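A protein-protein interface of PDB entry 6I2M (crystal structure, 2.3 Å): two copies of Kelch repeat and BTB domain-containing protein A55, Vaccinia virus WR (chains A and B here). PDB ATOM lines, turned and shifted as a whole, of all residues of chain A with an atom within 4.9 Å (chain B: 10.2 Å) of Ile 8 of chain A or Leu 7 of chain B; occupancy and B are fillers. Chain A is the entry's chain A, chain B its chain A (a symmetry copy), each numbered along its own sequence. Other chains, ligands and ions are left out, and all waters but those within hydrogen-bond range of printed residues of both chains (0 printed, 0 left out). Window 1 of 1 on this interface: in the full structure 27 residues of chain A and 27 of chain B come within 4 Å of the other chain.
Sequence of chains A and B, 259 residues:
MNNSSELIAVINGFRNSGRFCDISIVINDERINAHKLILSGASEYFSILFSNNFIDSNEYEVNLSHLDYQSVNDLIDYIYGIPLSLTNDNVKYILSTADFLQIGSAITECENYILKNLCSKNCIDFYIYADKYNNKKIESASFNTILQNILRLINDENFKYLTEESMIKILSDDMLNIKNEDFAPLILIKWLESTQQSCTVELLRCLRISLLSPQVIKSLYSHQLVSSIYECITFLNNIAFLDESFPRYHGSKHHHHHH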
ATOM      1  N   SER A   4      11.598   6.100  -1.060  1.00  0.00           N
ATOM      2  CA  SER A   4      11.031   6.248   0.280  1.00  0.00           C
ATOM      3  C   SER A   4      11.220   4.965   1.100  1.00  0.00           C
ATOM      4  O   SER A   4      11.539   5.039   2.289  1.00  0.00           O
ATOM      5  CB  SER A   4       9.554   6.614   0.189  1.00  0.00           C
ATOM      6  OG  SER A   4       9.070   7.111   1.424  1.00  0.00           O
ATOM      7  N   SER A   5      11.043   3.795   0.450  1.00  0.00           N
ATOM      8  CA  SER A   5      11.197   2.468   1.054  1.00  0.00           C
ATOM      9  C   SER A   5      12.667   2.146   1.350  1.00  0.00           C
ATOM     10  O   SER A   5      12.951   1.410   2.296  1.00  0.00           O
ATOM     11  CB  SER A   5      10.595   1.397   0.149  1.00  0.00           C
ATOM     12  OG  SER A   5       9.217   1.635  -0.089  1.00  0.00           O
ATOM     13  N   GLU A   6      13.592   2.691   0.538  1.00  0.00           N
ATOM     14  CA  GLU A   6      15.036   2.506   0.701  1.00  0.00           C
ATOM     15  C   GLU A   6      15.551   3.347   1.869  1.00  0.00           C
ATOM     16  O   GLU A   6      16.370   2.861   2.648  1.00  0.00           O
ATOM     17  CB  GLU A   6      15.785   2.882  -0.588  1.00  0.00           C
ATOM     18  CG  GLU A   6      15.628   1.880  -1.720  1.00  0.00           C
ATOM     19  CD  GLU A   6      16.007   2.382  -3.102  1.00  0.00           C
ATOM     20  OE1 GLU A   6      16.925   3.228  -3.208  1.00  0.00           O
ATOM     21  OE2 GLU A   6      15.388   1.917  -4.086  1.00  0.00           O
ATOM     22  N   LEU A   7      15.066   4.606   1.987  1.00  0.00           N
ATOM     23  CA  LEU A   7      15.438   5.566   3.031  1.00  0.00           C
ATOM     24  C   LEU A   7      15.048   5.093   4.439  1.00  0.00           C
ATOM     25  O   LEU A   7      15.871   5.185   5.352  1.00  0.00           O
ATOM     26  CB  LEU A   7      14.839   6.957   2.723  1.00  0.00           C
ATOM     27  CG  LEU A   7      15.132   8.088   3.721  1.00  0.00           C
ATOM     28  CD1 LEU A   7      16.495   8.704   3.487  1.00  0.00           C
ATOM     29  CD2 LEU A   7      14.077   9.156   3.649  1.00  0.00           C
ATOM     30  N   ILE A   8      13.807   4.587   4.606  1.00  0.00           N
ATOM     31  CA  ILE A   8      13.274   4.086   5.880  1.00  0.00           C
ATOM     32  C   ILE A   8      14.060   2.850   6.381  1.00  0.00           C
ATOM     33  O   ILE A   8      14.184   2.661   7.593  1.00  0.00           O
ATOM     34  CB  ILE A   8      11.730   3.857   5.806  1.00  0.00           C
ATOM     35  CG1 ILE A   8      11.098   3.736   7.216  1.00  0.00           C
ATOM     36  CG2 ILE A   8      11.339   2.678   4.888  1.00  0.00           C
ATOM     37  CD1 ILE A   8       9.585   3.920   7.266  1.00  0.00           C
ATOM     38  N   ALA A   9      14.611   2.044   5.446  1.00  0.00           N
ATOM     39  CA  ALA A   9      15.408   0.853   5.745  1.00  0.00           C
ATOM     40  C   ALA A   9      16.750   1.232   6.380  1.00  0.00           C
ATOM     41  O   ALA A   9      17.226   0.516   7.262  1.00  0.00           O
ATOM     42  CB  ALA A   9      15.636   0.043   4.477  1.00  0.00           C
ATOM     43  N   VAL A  10      17.343   2.365   5.941  1.00  0.00           N
ATOM     44  CA  VAL A  10      18.612   2.891   6.466  1.00  0.00           C
ATOM     45  C   VAL A  10      18.363   3.499   7.862  1.00  0.00           C
ATOM     46  O   VAL A  10      19.188   3.318   8.761  1.00  0.00           O
ATOM     47  CB  VAL A  10      19.312   3.884   5.489  1.00  0.00           C
ATOM     48  CG1 VAL A  10      20.719   4.235   5.967  1.00  0.00           C
ATOM     49  CG2 VAL A  10      19.371   3.322   4.070  1.00  0.00           C
ATOM     50  N   ILE A  11      17.206   4.185   8.042  1.00  0.00           N
ATOM     51  CA  ILE A  11      16.768   4.797   9.308  1.00  0.00           C
ATOM     52  C   ILE A  11      16.521   3.690  10.355  1.00  0.00           C
ATOM     53  O   ILE A  11      16.932   3.841  11.509  1.00  0.00           O
ATOM     54  CB  ILE A  11      15.548   5.752   9.092  1.00  0.00           C
ATOM     55  CG1 ILE A  11      15.949   6.968   8.221  1.00  0.00           C
ATOM     56  CG2 ILE A  11      14.925   6.216  10.423  1.00  0.00           C
ATOM     57  CD1 ILE A  11      14.792   7.686   7.510  1.00  0.00           C
ATOM     58  N   ASN A  12      15.906   2.562   9.928  1.00  0.00           N
ATOM     59  CA  ASN A  12      15.654   1.390  10.777  1.00  0.00           C
ATOM     60  C   ASN A  12      16.978   0.704  11.138  1.00  0.00           C
ATOM     61  O   ASN A  12      17.084   0.107  12.209  1.00  0.00           O
ATOM     62  CB  ASN A  12      14.695   0.407  10.092  1.00  0.00           C
ATOM     63  CG  ASN A  12      14.229  -0.742  10.963  1.00  0.00           C
ATOM     64  OD1 ASN A  12      13.790  -0.566  12.108  1.00  0.00           O
ATOM     65  ND2 ASN A  12      14.298  -1.950  10.425  1.00  0.00           N
ATOM     66  N   ILE A  38      10.488  10.442  13.655  1.00  0.00           N
ATOM     67  CA  ILE A  38       9.870   9.252  13.054  1.00  0.00           C
ATOM     68  C   ILE A  38       8.550   8.883  13.756  1.00  0.00           C
ATOM     69  O   ILE A  38       7.550   8.653  13.072  1.00  0.00           O
ATOM     70  CB  ILE A  38      10.886   8.061  12.981  1.00  0.00           C
ATOM     71  CG1 ILE A  38      12.215   8.452  12.270  1.00  0.00           C
ATOM     72  CG2 ILE A  38      10.275   6.793  12.367  1.00  0.00           C
ATOM     73  CD1 ILE A  38      12.147   8.894  10.731  1.00  0.00           C
ATOM     74  N   GLY A  41       5.710  11.477  13.032  1.00  0.00           N
ATOM     75  CA  GLY A  41       5.219  11.414  11.659  1.00  0.00           C
ATOM     76  C   GLY A  41       4.045  10.476  11.445  1.00  0.00           C
ATOM     77  O   GLY A  41       3.117  10.811  10.702  1.00  0.00           O
ATOM     78  N   ALA A  42       4.082   9.290  12.083  1.00  0.00           N
ATOM     79  CA  ALA A  42       3.034   8.272  11.970  1.00  0.00           C
ATOM     80  C   ALA A  42       2.009   8.355  13.102  1.00  0.00           C
ATOM     81  O   ALA A  42       0.808   8.279  12.836  1.00  0.00           O
ATOM     82  CB  ALA A  42       3.651   6.884  11.915  1.00  0.00           C
ATOM     83  N   ILE A  79       5.883   1.585  12.149  1.00  0.00           N
ATOM     84  CA  ILE A  79       6.231   2.990  11.869  1.00  0.00           C
ATOM     85  C   ILE A  79       7.494   2.986  10.983  1.00  0.00           C
ATOM     86  O   ILE A  79       7.599   3.785  10.051  1.00  0.00           O
ATOM     87  CB  ILE A  79       6.386   3.831  13.183  1.00  0.00           C
ATOM     88  CG1 ILE A  79       5.035   3.967  13.920  1.00  0.00           C
ATOM     89  CG2 ILE A  79       6.980   5.221  12.915  1.00  0.00           C
ATOM     90  CD1 ILE A  79       5.107   4.206  15.441  1.00  0.00           C
ATOM     91  N   TYR A  80       8.411   2.030  11.246  1.00  0.00           N
ATOM     92  CA  TYR A  80       9.634   1.810  10.476  1.00  0.00           C
ATOM     93  C   TYR A  80       9.343   0.870   9.275  1.00  0.00           C
ATOM     94  O   TYR A  80       8.175   0.603   8.981  1.00  0.00           O
ATOM     95  CB  TYR A  80      10.769   1.301  11.390  1.00  0.00           C
ATOM     96  CG  TYR A  80      11.339   2.373  12.300  1.00  0.00           C
ATOM     97  CD1 TYR A  80      10.735   2.677  13.516  1.00  0.00           C
ATOM     98  CD2 TYR A  80      12.491   3.071  11.951  1.00  0.00           C
ATOM     99  CE1 TYR A  80      11.248   3.666  14.353  1.00  0.00           C
ATOM    100  CE2 TYR A  80      13.022   4.056  12.786  1.00  0.00           C
ATOM    101  CZ  TYR A  80      12.397   4.348  13.988  1.00  0.00           C
ATOM    102  OH  TYR A  80      12.907   5.317  14.817  1.00  0.00           O
ATOM    103  N   GLY A  81      10.388   0.407   8.586  1.00  0.00           N
ATOM    104  CA  GLY A  81      10.266  -0.425   7.390  1.00  0.00           C
ATOM    105  C   GLY A  81       9.830  -1.874   7.534  1.00  0.00           C
ATOM    106  O   GLY A  81       9.976  -2.639   6.578  1.00  0.00           O
ATOM    107  N   MET B   1      -0.411  -2.846   4.003  1.00  0.00           N
ATOM    108  CA  MET B   1      -0.158  -1.646   3.208  1.00  0.00           C
ATOM    109  C   MET B   1       1.177  -0.970   3.561  1.00  0.00           C
ATOM    110  O   MET B   1       1.666  -1.119   4.684  1.00  0.00           O
ATOM    111  CB  MET B   1      -1.338  -0.649   3.302  1.00  0.00           C
ATOM    112  CG  MET B   1      -1.504   0.005   4.671  1.00  0.00           C
ATOM    113  SD  MET B   1      -2.878   1.176   4.760  1.00  0.00           S
ATOM    114  CE  MET B   1      -4.215   0.066   5.162  1.00  0.00           C
ATOM    115  N   ASN B   2       1.754  -0.229   2.598  1.00  0.00           N
ATOM    116  CA  ASN B   2       3.003   0.510   2.784  1.00  0.00           C
ATOM    117  C   ASN B   2       2.681   1.991   2.986  1.00  0.00           C
ATOM    118  O   ASN B   2       2.036   2.608   2.131  1.00  0.00           O
ATOM    119  CB  ASN B   2       3.965   0.296   1.603  1.00  0.00           C
ATOM    120  CG  ASN B   2       5.340   0.909   1.781  1.00  0.00           C
ATOM    121  OD1 ASN B   2       5.896   0.978   2.885  1.00  0.00           O
ATOM    122  ND2 ASN B   2       5.930   1.357   0.683  1.00  0.00           N
ATOM    123  N   ASN B   3       3.101   2.543   4.135  1.00  0.00           N
ATOM    124  CA  ASN B   3       2.853   3.937   4.506  1.00  0.00           C
ATOM    125  C   ASN B   3       4.152   4.753   4.584  1.00  0.00           C
ATOM    126  O   ASN B   3       4.221   5.757   5.301  1.00  0.00           O
ATOM    127  CB  ASN B   3       2.053   4.007   5.813  1.00  0.00           C
ATOM    128  CG  ASN B   3       0.803   3.164   5.798  1.00  0.00           C
ATOM    129  OD1 ASN B   3       0.810   1.997   6.201  1.00  0.00           O
ATOM    130  ND2 ASN B   3      -0.299   3.736   5.336  1.00  0.00           N
ATOM    131  N   SER B   4       5.173   4.328   3.816  1.00  0.00           N
ATOM    132  CA  SER B   4       6.483   4.975   3.743  1.00  0.00           C
ATOM    133  C   SER B   4       6.380   6.350   3.068  1.00  0.00           C
ATOM    134  O   SER B   4       7.021   7.303   3.519  1.00  0.00           O
ATOM    135  CB  SER B   4       7.469   4.084   2.996  1.00  0.00           C
ATOM    136  OG  SER B   4       8.806   4.499   3.216  1.00  0.00           O
ATOM    137  N   SER B   5       5.552   6.446   2.006  1.00  0.00           N
ATOM    138  CA  SER B   5       5.306   7.674   1.243  1.00  0.00           C
ATOM    139  C   SER B   5       4.481   8.685   2.048  1.00  0.00           C
ATOM    140  O   SER B   5       4.636   9.891   1.852  1.00  0.00           O
ATOM    141  CB  SER B   5       4.605   7.351  -0.073  1.00  0.00           C
ATOM    142  OG  SER B   5       5.378   6.467  -0.868  1.00  0.00           O
ATOM    143  N   GLU B   6       3.604   8.192   2.943  1.00  0.00           N
ATOM    144  CA  GLU B   6       2.762   9.022   3.808  1.00  0.00           C
ATOM    145  C   GLU B   6       3.596   9.623   4.940  1.00  0.00           C
ATOM    146  O   GLU B   6       3.421  10.798   5.260  1.00  0.00           O
ATOM    147  CB  GLU B   6       1.599   8.203   4.390  1.00  0.00           C
ATOM    148  CG  GLU B   6       0.506   7.867   3.388  1.00  0.00           C
ATOM    149  CD  GLU B   6      -0.444   6.755   3.797  1.00  0.00           C
ATOM    150  OE1 GLU B   6      -0.712   6.604   5.012  1.00  0.00           O
ATOM    151  OE2 GLU B   6      -0.930   6.037   2.894  1.00  0.00           O
ATOM    152  N   LEU B   7       4.501   8.814   5.540  1.00  0.00           N
ATOM    153  CA  LEU B   7       5.387   9.200   6.643  1.00  0.00           C
ATOM    154  C   LEU B   7       6.373  10.310   6.252  1.00  0.00           C
ATOM    155  O   LEU B   7       6.531  11.267   7.013  1.00  0.00           O
ATOM    156  CB  LEU B   7       6.130   7.962   7.197  1.00  0.00           C
ATOM    157  CG  LEU B   7       7.105   8.187   8.362  1.00  0.00           C
ATOM    158  CD1 LEU B   7       6.384   8.258   9.692  1.00  0.00           C
ATOM    159  CD2 LEU B   7       8.146   7.105   8.411  1.00  0.00           C
ATOM    160  N   ILE B   8       7.022  10.183   5.074  1.00  0.00           N
ATOM    161  CA  ILE B   8       7.992  11.152   4.546  1.00  0.00           C
ATOM    162  C   ILE B   8       7.332  12.522   4.260  1.00  0.00           C
ATOM    163  O   ILE B   8       7.995  13.553   4.391  1.00  0.00           O
ATOM    164  CB  ILE B   8       8.779  10.570   3.328  1.00  0.00           C
ATOM    165  CG1 ILE B   8      10.060  11.387   3.028  1.00  0.00           C
ATOM    166  CG2 ILE B   8       7.896  10.387   2.073  1.00  0.00           C
ATOM    167  CD1 ILE B   8      11.087  10.682   2.147  1.00  0.00           C
ATOM    168  N   ALA B   9       6.027  12.521   3.908  1.00  0.00           N
ATOM    169  CA  ALA B   9       5.243  13.726   3.632  1.00  0.00           C
ATOM    170  C   ALA B   9       5.021  14.544   4.908  1.00  0.00           C
ATOM    171  O   ALA B   9       5.026  15.775   4.846  1.00  0.00           O
ATOM    172  CB  ALA B   9       3.907  13.350   3.008  1.00  0.00           C
ATOM    173  N   VAL B  10       4.846  13.859   6.059  1.00  0.00           N
ATOM    174  CA  VAL B  10       4.656  14.487   7.375  1.00  0.00           C
ATOM    175  C   VAL B  10       6.006  15.057   7.858  1.00  0.00           C
ATOM    176  O   VAL B  10       6.037  16.154   8.421  1.00  0.00           O
ATOM    177  CB  VAL B  10       3.993  13.534   8.417  1.00  0.00           C
ATOM    178  CG1 VAL B  10       3.614  14.283   9.693  1.00  0.00           C
ATOM    179  CG2 VAL B  10       2.762  12.842   7.835  1.00  0.00           C
ATOM    180  N   ILE B  11       7.116  14.322   7.600  1.00  0.00           N
ATOM    181  CA  ILE B  11       8.495  14.715   7.938  1.00  0.00           C
ATOM    182  C   ILE B  11       8.882  15.973   7.131  1.00  0.00           C
ATOM    183  O   ILE B  11       9.478  16.897   7.693  1.00  0.00           O
ATOM    184  CB  ILE B  11       9.490  13.521   7.772  1.00  0.00           C
ATOM    185  CG1 ILE B  11       9.175  12.396   8.788  1.00  0.00           C
ATOM    186  CG2 ILE B  11      10.962  13.964   7.889  1.00  0.00           C
ATOM    187  CD1 ILE B  11       9.698  11.000   8.418  1.00  0.00           C
ATOM    188  N   ASN B  12       8.489  16.022   5.837  1.00  0.00           N
ATOM    189  CA  ASN B  12       8.719  17.170   4.950  1.00  0.00           C
ATOM    190  C   ASN B  12       7.871  18.366   5.402  1.00  0.00           C
ATOM    191  O   ASN B  12       8.277  19.511   5.206  1.00  0.00           O
ATOM    192  CB  ASN B  12       8.419  16.808   3.489  1.00  0.00           C
ATOM    193  CG  ASN B  12       8.803  17.868   2.476  1.00  0.00           C
ATOM    194  OD1 ASN B  12       9.915  18.413   2.481  1.00  0.00           O
ATOM    195  ND2 ASN B  12       7.887  18.170   1.570  1.00  0.00           N
ATOM    196  N   GLY B  13       6.719  18.074   6.011  1.00  0.00           N
ATOM    197  CA  GLY B  13       5.808  19.065   6.573  1.00  0.00           C
ATOM    198  C   GLY B  13       6.391  19.688   7.828  1.00  0.00           C
ATOM    199  O   GLY B  13       6.196  20.880   8.076  1.00  0.00           O
ATOM    200  N   PHE B  14       7.127  18.872   8.620  1.00  0.00           N
ATOM    201  CA  PHE B  14       7.821  19.293   9.840  1.00  0.00           C
ATOM    202  C   PHE B  14       9.051  20.131   9.469  1.00  0.00           C
ATOM    203  O   PHE B  14       9.393  21.067  10.190  1.00  0.00           O
ATOM    204  CB  PHE B  14       8.264  18.075  10.677  1.00  0.00           C
ATOM    205  CG  PHE B  14       7.196  17.238  11.352  1.00  0.00           C
ATOM    206  CD1 PHE B  14       6.088  17.834  11.946  1.00  0.00           C
ATOM    207  CD2 PHE B  14       7.349  15.862  11.480  1.00  0.00           C
ATOM    208  CE1 PHE B  14       5.120  17.061  12.595  1.00  0.00           C
ATOM    209  CE2 PHE B  14       6.386  15.091  12.137  1.00  0.00           C
ATOM    210  CZ  PHE B  14       5.279  15.696  12.692  1.00  0.00           C
ATOM    211  N   ARG B  15       9.711  19.781   8.341  1.00  0.00           N
ATOM    212  CA  ARG B  15      10.893  20.446   7.787  1.00  0.00           C
ATOM    213  C   ARG B  15      10.576  21.902   7.408  1.00  0.00           C
ATOM    214  O   ARG B  15      11.366  22.797   7.715  1.00  0.00           O
ATOM    215  CB  ARG B  15      11.412  19.652   6.572  1.00  0.00           C
ATOM    216  CG  ARG B  15      12.637  20.239   5.876  1.00  0.00           C
ATOM    217  CD  ARG B  15      12.721  19.741   4.449  1.00  0.00           C
ATOM    218  NE  ARG B  15      13.579  20.586   3.619  1.00  0.00           N
ATOM    219  CZ  ARG B  15      13.616  20.543   2.289  1.00  0.00           C
ATOM    220  NH1 ARG B  15      12.838  19.697   1.623  1.00  0.00           N
ATOM    221  NH2 ARG B  15      14.426  21.349   1.617  1.00  0.00           N
ATOM    222  N   PHE B  20      11.695  19.707  14.754  1.00  0.00           N
ATOM    223  CA  PHE B  20      12.745  18.686  14.929  1.00  0.00           C
ATOM    224  C   PHE B  20      14.054  18.964  14.154  1.00  0.00           C
ATOM    225  O   PHE B  20      14.981  18.151  14.233  1.00  0.00           O
ATOM    226  CB  PHE B  20      12.219  17.268  14.612  1.00  0.00           C
ATOM    227  CG  PHE B  20      10.964  16.868  15.347  1.00  0.00           C
ATOM    228  CD1 PHE B  20      11.027  16.364  16.641  1.00  0.00           C
ATOM    229  CD2 PHE B  20       9.719  16.968  14.737  1.00  0.00           C
ATOM    230  CE1 PHE B  20       9.865  15.984  17.318  1.00  0.00           C
ATOM    231  CE2 PHE B  20       8.559  16.589  15.414  1.00  0.00           C
ATOM    232  CZ  PHE B  20       8.640  16.103  16.701  1.00  0.00           C
ATOM    233  N   HIS B  35      16.914  17.661   8.897  1.00  0.00           N
ATOM    234  CA  HIS B  35      17.140  16.724   9.999  1.00  0.00           C
ATOM    235  C   HIS B  35      18.385  15.876   9.715  1.00  0.00           C
ATOM    236  O   HIS B  35      18.563  15.413   8.584  1.00  0.00           O
ATOM    237  CB  HIS B  35      15.904  15.830  10.207  1.00  0.00           C
ATOM    238  CG  HIS B  35      14.623  16.597  10.328  1.00  0.00           C
ATOM    239  ND1 HIS B  35      13.970  17.093   9.213  1.00  0.00           N
ATOM    240  CD2 HIS B  35      13.918  16.937  11.431  1.00  0.00           C
ATOM    241  CE1 HIS B  35      12.895  17.713   9.670  1.00  0.00           C
ATOM    242  NE2 HIS B  35      12.823  17.649  10.999  1.00  0.00           N
ATOM    243  N   LEU B  37      19.259  12.813  10.721  1.00  0.00           N
ATOM    244  CA  LEU B  37      18.891  11.427  10.433  1.00  0.00           C
ATOM    245  C   LEU B  37      18.469  11.208   8.972  1.00  0.00           C
ATOM    246  O   LEU B  37      18.909  10.235   8.355  1.00  0.00           O
ATOM    247  CB  LEU B  37      17.780  10.991  11.413  1.00  0.00           C
ATOM    248  CG  LEU B  37      17.044   9.679  11.155  1.00  0.00           C
ATOM    249  CD1 LEU B  37      17.864   8.479  11.610  1.00  0.00           C
ATOM    250  CD2 LEU B  37      15.712   9.682  11.852  1.00  0.00           C
ATOM    251  N   ILE B  38      17.614  12.107   8.436  1.00  0.00           N
ATOM    252  CA  ILE B  38      17.078  12.064   7.068  1.00  0.00           C
ATOM    253  C   ILE B  38      18.194  12.213   6.017  1.00  0.00           C
ATOM    254  O   ILE B  38      18.239  11.423   5.072  1.00  0.00           O
ATOM    255  CB  ILE B  38      15.910  13.092   6.882  1.00  0.00           C
ATOM    256  CG1 ILE B  38      14.792  12.927   7.954  1.00  0.00           C
ATOM    257  CG2 ILE B  38      15.329  13.085   5.461  1.00  0.00           C
ATOM    258  CD1 ILE B  38      13.982  11.545   7.994  1.00  0.00           C
ATOM    259  N   SER B  40      21.415  11.629   6.454  1.00  0.00           N
ATOM    260  CA  SER B  40      22.339  10.505   6.627  1.00  0.00           C
ATOM    261  C   SER B  40      21.840   9.204   5.984  1.00  0.00           C
ATOM    262  O   SER B  40      22.655   8.360   5.605  1.00  0.00           O
ATOM    263  CB  SER B  40      22.639  10.290   8.106  1.00  0.00           C
ATOM    264  OG  SER B  40      23.353  11.396   8.634  1.00  0.00           O
ATOM    265  N   GLY B  41      20.519   9.070   5.864  1.00  0.00           N
ATOM    266  CA  GLY B  41      19.863   7.904   5.278  1.00  0.00           C
ATOM    267  C   GLY B  41      20.031   7.767   3.776  1.00  0.00           C
ATOM    268  O   GLY B  41      20.232   6.654   3.279  1.00  0.00           O
ATOM    269  N   ALA B  42      19.937   8.892   3.041  1.00  0.00           N
ATOM    270  CA  ALA B  42      20.064   8.924   1.582  1.00  0.00           C
ATOM    271  C   ALA B  42      21.482   9.262   1.121  1.00  0.00           C
ATOM    272  O   ALA B  42      21.997   8.604   0.216  1.00  0.00           O
ATOM    273  CB  ALA B  42      19.066   9.905   0.988  1.00  0.00           C
ATOM    274  N   ILE B  79      15.633  13.919  -1.297  1.00  0.00           N
ATOM    275  CA  ILE B  79      15.828  13.096  -0.090  1.00  0.00           C
ATOM    276  C   ILE B  79      14.465  12.993   0.626  1.00  0.00           C
ATOM    277  O   ILE B  79      14.111  11.926   1.132  1.00  0.00           O
ATOM    278  CB  ILE B  79      16.977  13.649   0.821  1.00  0.00           C
ATOM    279  CG1 ILE B  79      18.349  13.535   0.119  1.00  0.00           C
ATOM    280  CG2 ILE B  79      17.025  12.946   2.185  1.00  0.00           C
ATOM    281  CD1 ILE B  79      19.433  14.533   0.572  1.00  0.00           C
ATOM    282  N   TYR B  80      13.683  14.093   0.594  1.00  0.00           N
ATOM    283  CA  TYR B  80      12.331  14.175   1.144  1.00  0.00           C
ATOM    284  C   TYR B  80      11.299  13.699   0.087  1.00  0.00           C
ATOM    285  O   TYR B  80      11.694  13.139  -0.940  1.00  0.00           O
ATOM    286  CB  TYR B  80      12.047  15.594   1.681  1.00  0.00           C
ATOM    287  CG  TYR B  80      12.770  15.906   2.978  1.00  0.00           C
ATOM    288  CD1 TYR B  80      14.085  16.361   2.975  1.00  0.00           C
ATOM    289  CD2 TYR B  80      12.133  15.759   4.207  1.00  0.00           C
ATOM    290  CE1 TYR B  80      14.758  16.641   4.162  1.00  0.00           C
ATOM    291  CE2 TYR B  80      12.793  16.048   5.402  1.00  0.00           C
ATOM    292  CZ  TYR B  80      14.106  16.491   5.374  1.00  0.00           C
ATOM    293  OH  TYR B  80      14.767  16.775   6.544  1.00  0.00           O
ATOM    294  N   GLY B  81      10.007  13.898   0.353  1.00  0.00           N
ATOM    295  CA  GLY B  81       8.921  13.438  -0.512  1.00  0.00           C
ATOM    296  C   GLY B  81       8.669  14.151  -1.831  1.00  0.00           C
ATOM    297  O   GLY B  81       7.611  13.940  -2.430  1.00  0.00           O
ATOM    298  N   SER B 105      20.593   7.164  -4.854  1.00  0.00           N
ATOM    299  CA  SER B 105      19.239   7.349  -5.375  1.00  0.00           C
ATOM    300  C   SER B 105      19.163   8.452  -6.436  1.00  0.00           C
ATOM    301  O   SER B 105      18.384   8.335  -7.384  1.00  0.00           O
ATOM    302  CB  SER B 105      18.282   7.662  -4.231  1.00  0.00           C
ATOM    303  OG  SER B 105      18.210   6.584  -3.312  1.00  0.00           O
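The backbone carbonyl oxygen (O) of Ser 4 of chain A lies within hydrogen-bond range of the side-chain hydroxyl (OG) of Ser 4 of chain B. OG of Ser 5 of chain A sits at hydrogen-bond distance from ND2 of Asn 2 of chain B (3.4 Å).
Ser 5 of chain B touches Ser 4 of chain A (N to OG, 3.6 Å). Ser 5 of chain A touches Ser 4 of chain B (N to OG, 3.6 Å). OE1 of Glu 6 of chain A touches OG of Ser 105 of chain B (3.6 Å). Leu 7 of chain A touches Ile 38 of chain B (CD1 to O, 3.6 Å). Leu 7 of chain A touches Ile 79 of chain B (CD2 to O, 3.7 Å). Ile 8 of chain A touches Leu 7 of chain B (CD1 to CD2, 3.7 Å). CG2 of Val 10 of chain A touches O of Gly 41 of chain B, 3.5 Å away. Ile 38 of chain A touches Leu 37 of chain B (CG1 to CD2, 3.7 Å). Leu 7 of chain B touches Gly 41 of chain A. Gly 41 of chain A touches Phe 14 of chain B (N to CE2, 3.8 Å).
Of chain B, only Ser 4 (3.5 Å) and Leu 7 (3.7 Å) come within 4 Å of Ile 8 of chain A. Leu 7 of chain B touches just these residues of chain A: Ile 8, Ile 38, Gly 41, Ala 42 and Ile 79. Leu 7 of chain A touches five residues of chain B. Of chain B, only Leu 37 (3.8 Å) and Ile 38 (3.97 Å) come within 4 Å of Ile 11 of chain A. Gly 41 of chain A touches just these residues of chain B: Leu 7, Val 10 and Phe 14. Gly 81 of chain A touches none of the printed residues of chain B. Printed residues of chain B within 4 Å of Ala 42 of chain A: Leu 7. Of the printed residues of chain A, Ile 79 of chain B touches Leu 7. Of the printed residues of chain A, Val 10 of chain B touches Gly 41. Of the printed residues of chain A, Ser 105 of chain B touches Glu 6. Gly 13 of chain B touches none of the printed residues of chain A. The nearest residue of chain B that does not touch Ile 8 of chain A is Asn 3 of chain B (6.0 Å).
Of the 15 printed residues of chain A, 11 touch a printed residue of chain B. Hydrophobic or aromatic side chains of chain A within 4 Å of the printed part of chain B: Leu 7, Ile 8, Val 10, Ile 11, Ile 38 and Ala 42. Hydrophobic or aromatic side chains of chain B within 4 Å of the printed part of chain A: Leu 7, Ile 8, Val 10, Ile 11, Phe 14, Leu 37, Ile 38 and Ala 42.
Ser 4 of chain A touches Ser 5 of chain B, and with the chains exchanged Ser 5 of chain A touches Ser 4 of chain B. Ser 4 of chain A touches Ile 8 of chain B, and with the chains exchanged Ile 8 of chain A touches Ser 4 of chain B. Leu 7 of chain A touches Ile 8 of chain B, and with the chains exchanged Ile 8 of chain A touches Leu 7 of chain B. Ile 11 of chain A touches Ile 38 of chain B, and with the chains exchanged Ile 38 of chain A touches Ile 11 of chain B. Of the 24 pairs that touch across the chains among the printed residues, 19 have their exchanged pair printed and touching as well.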
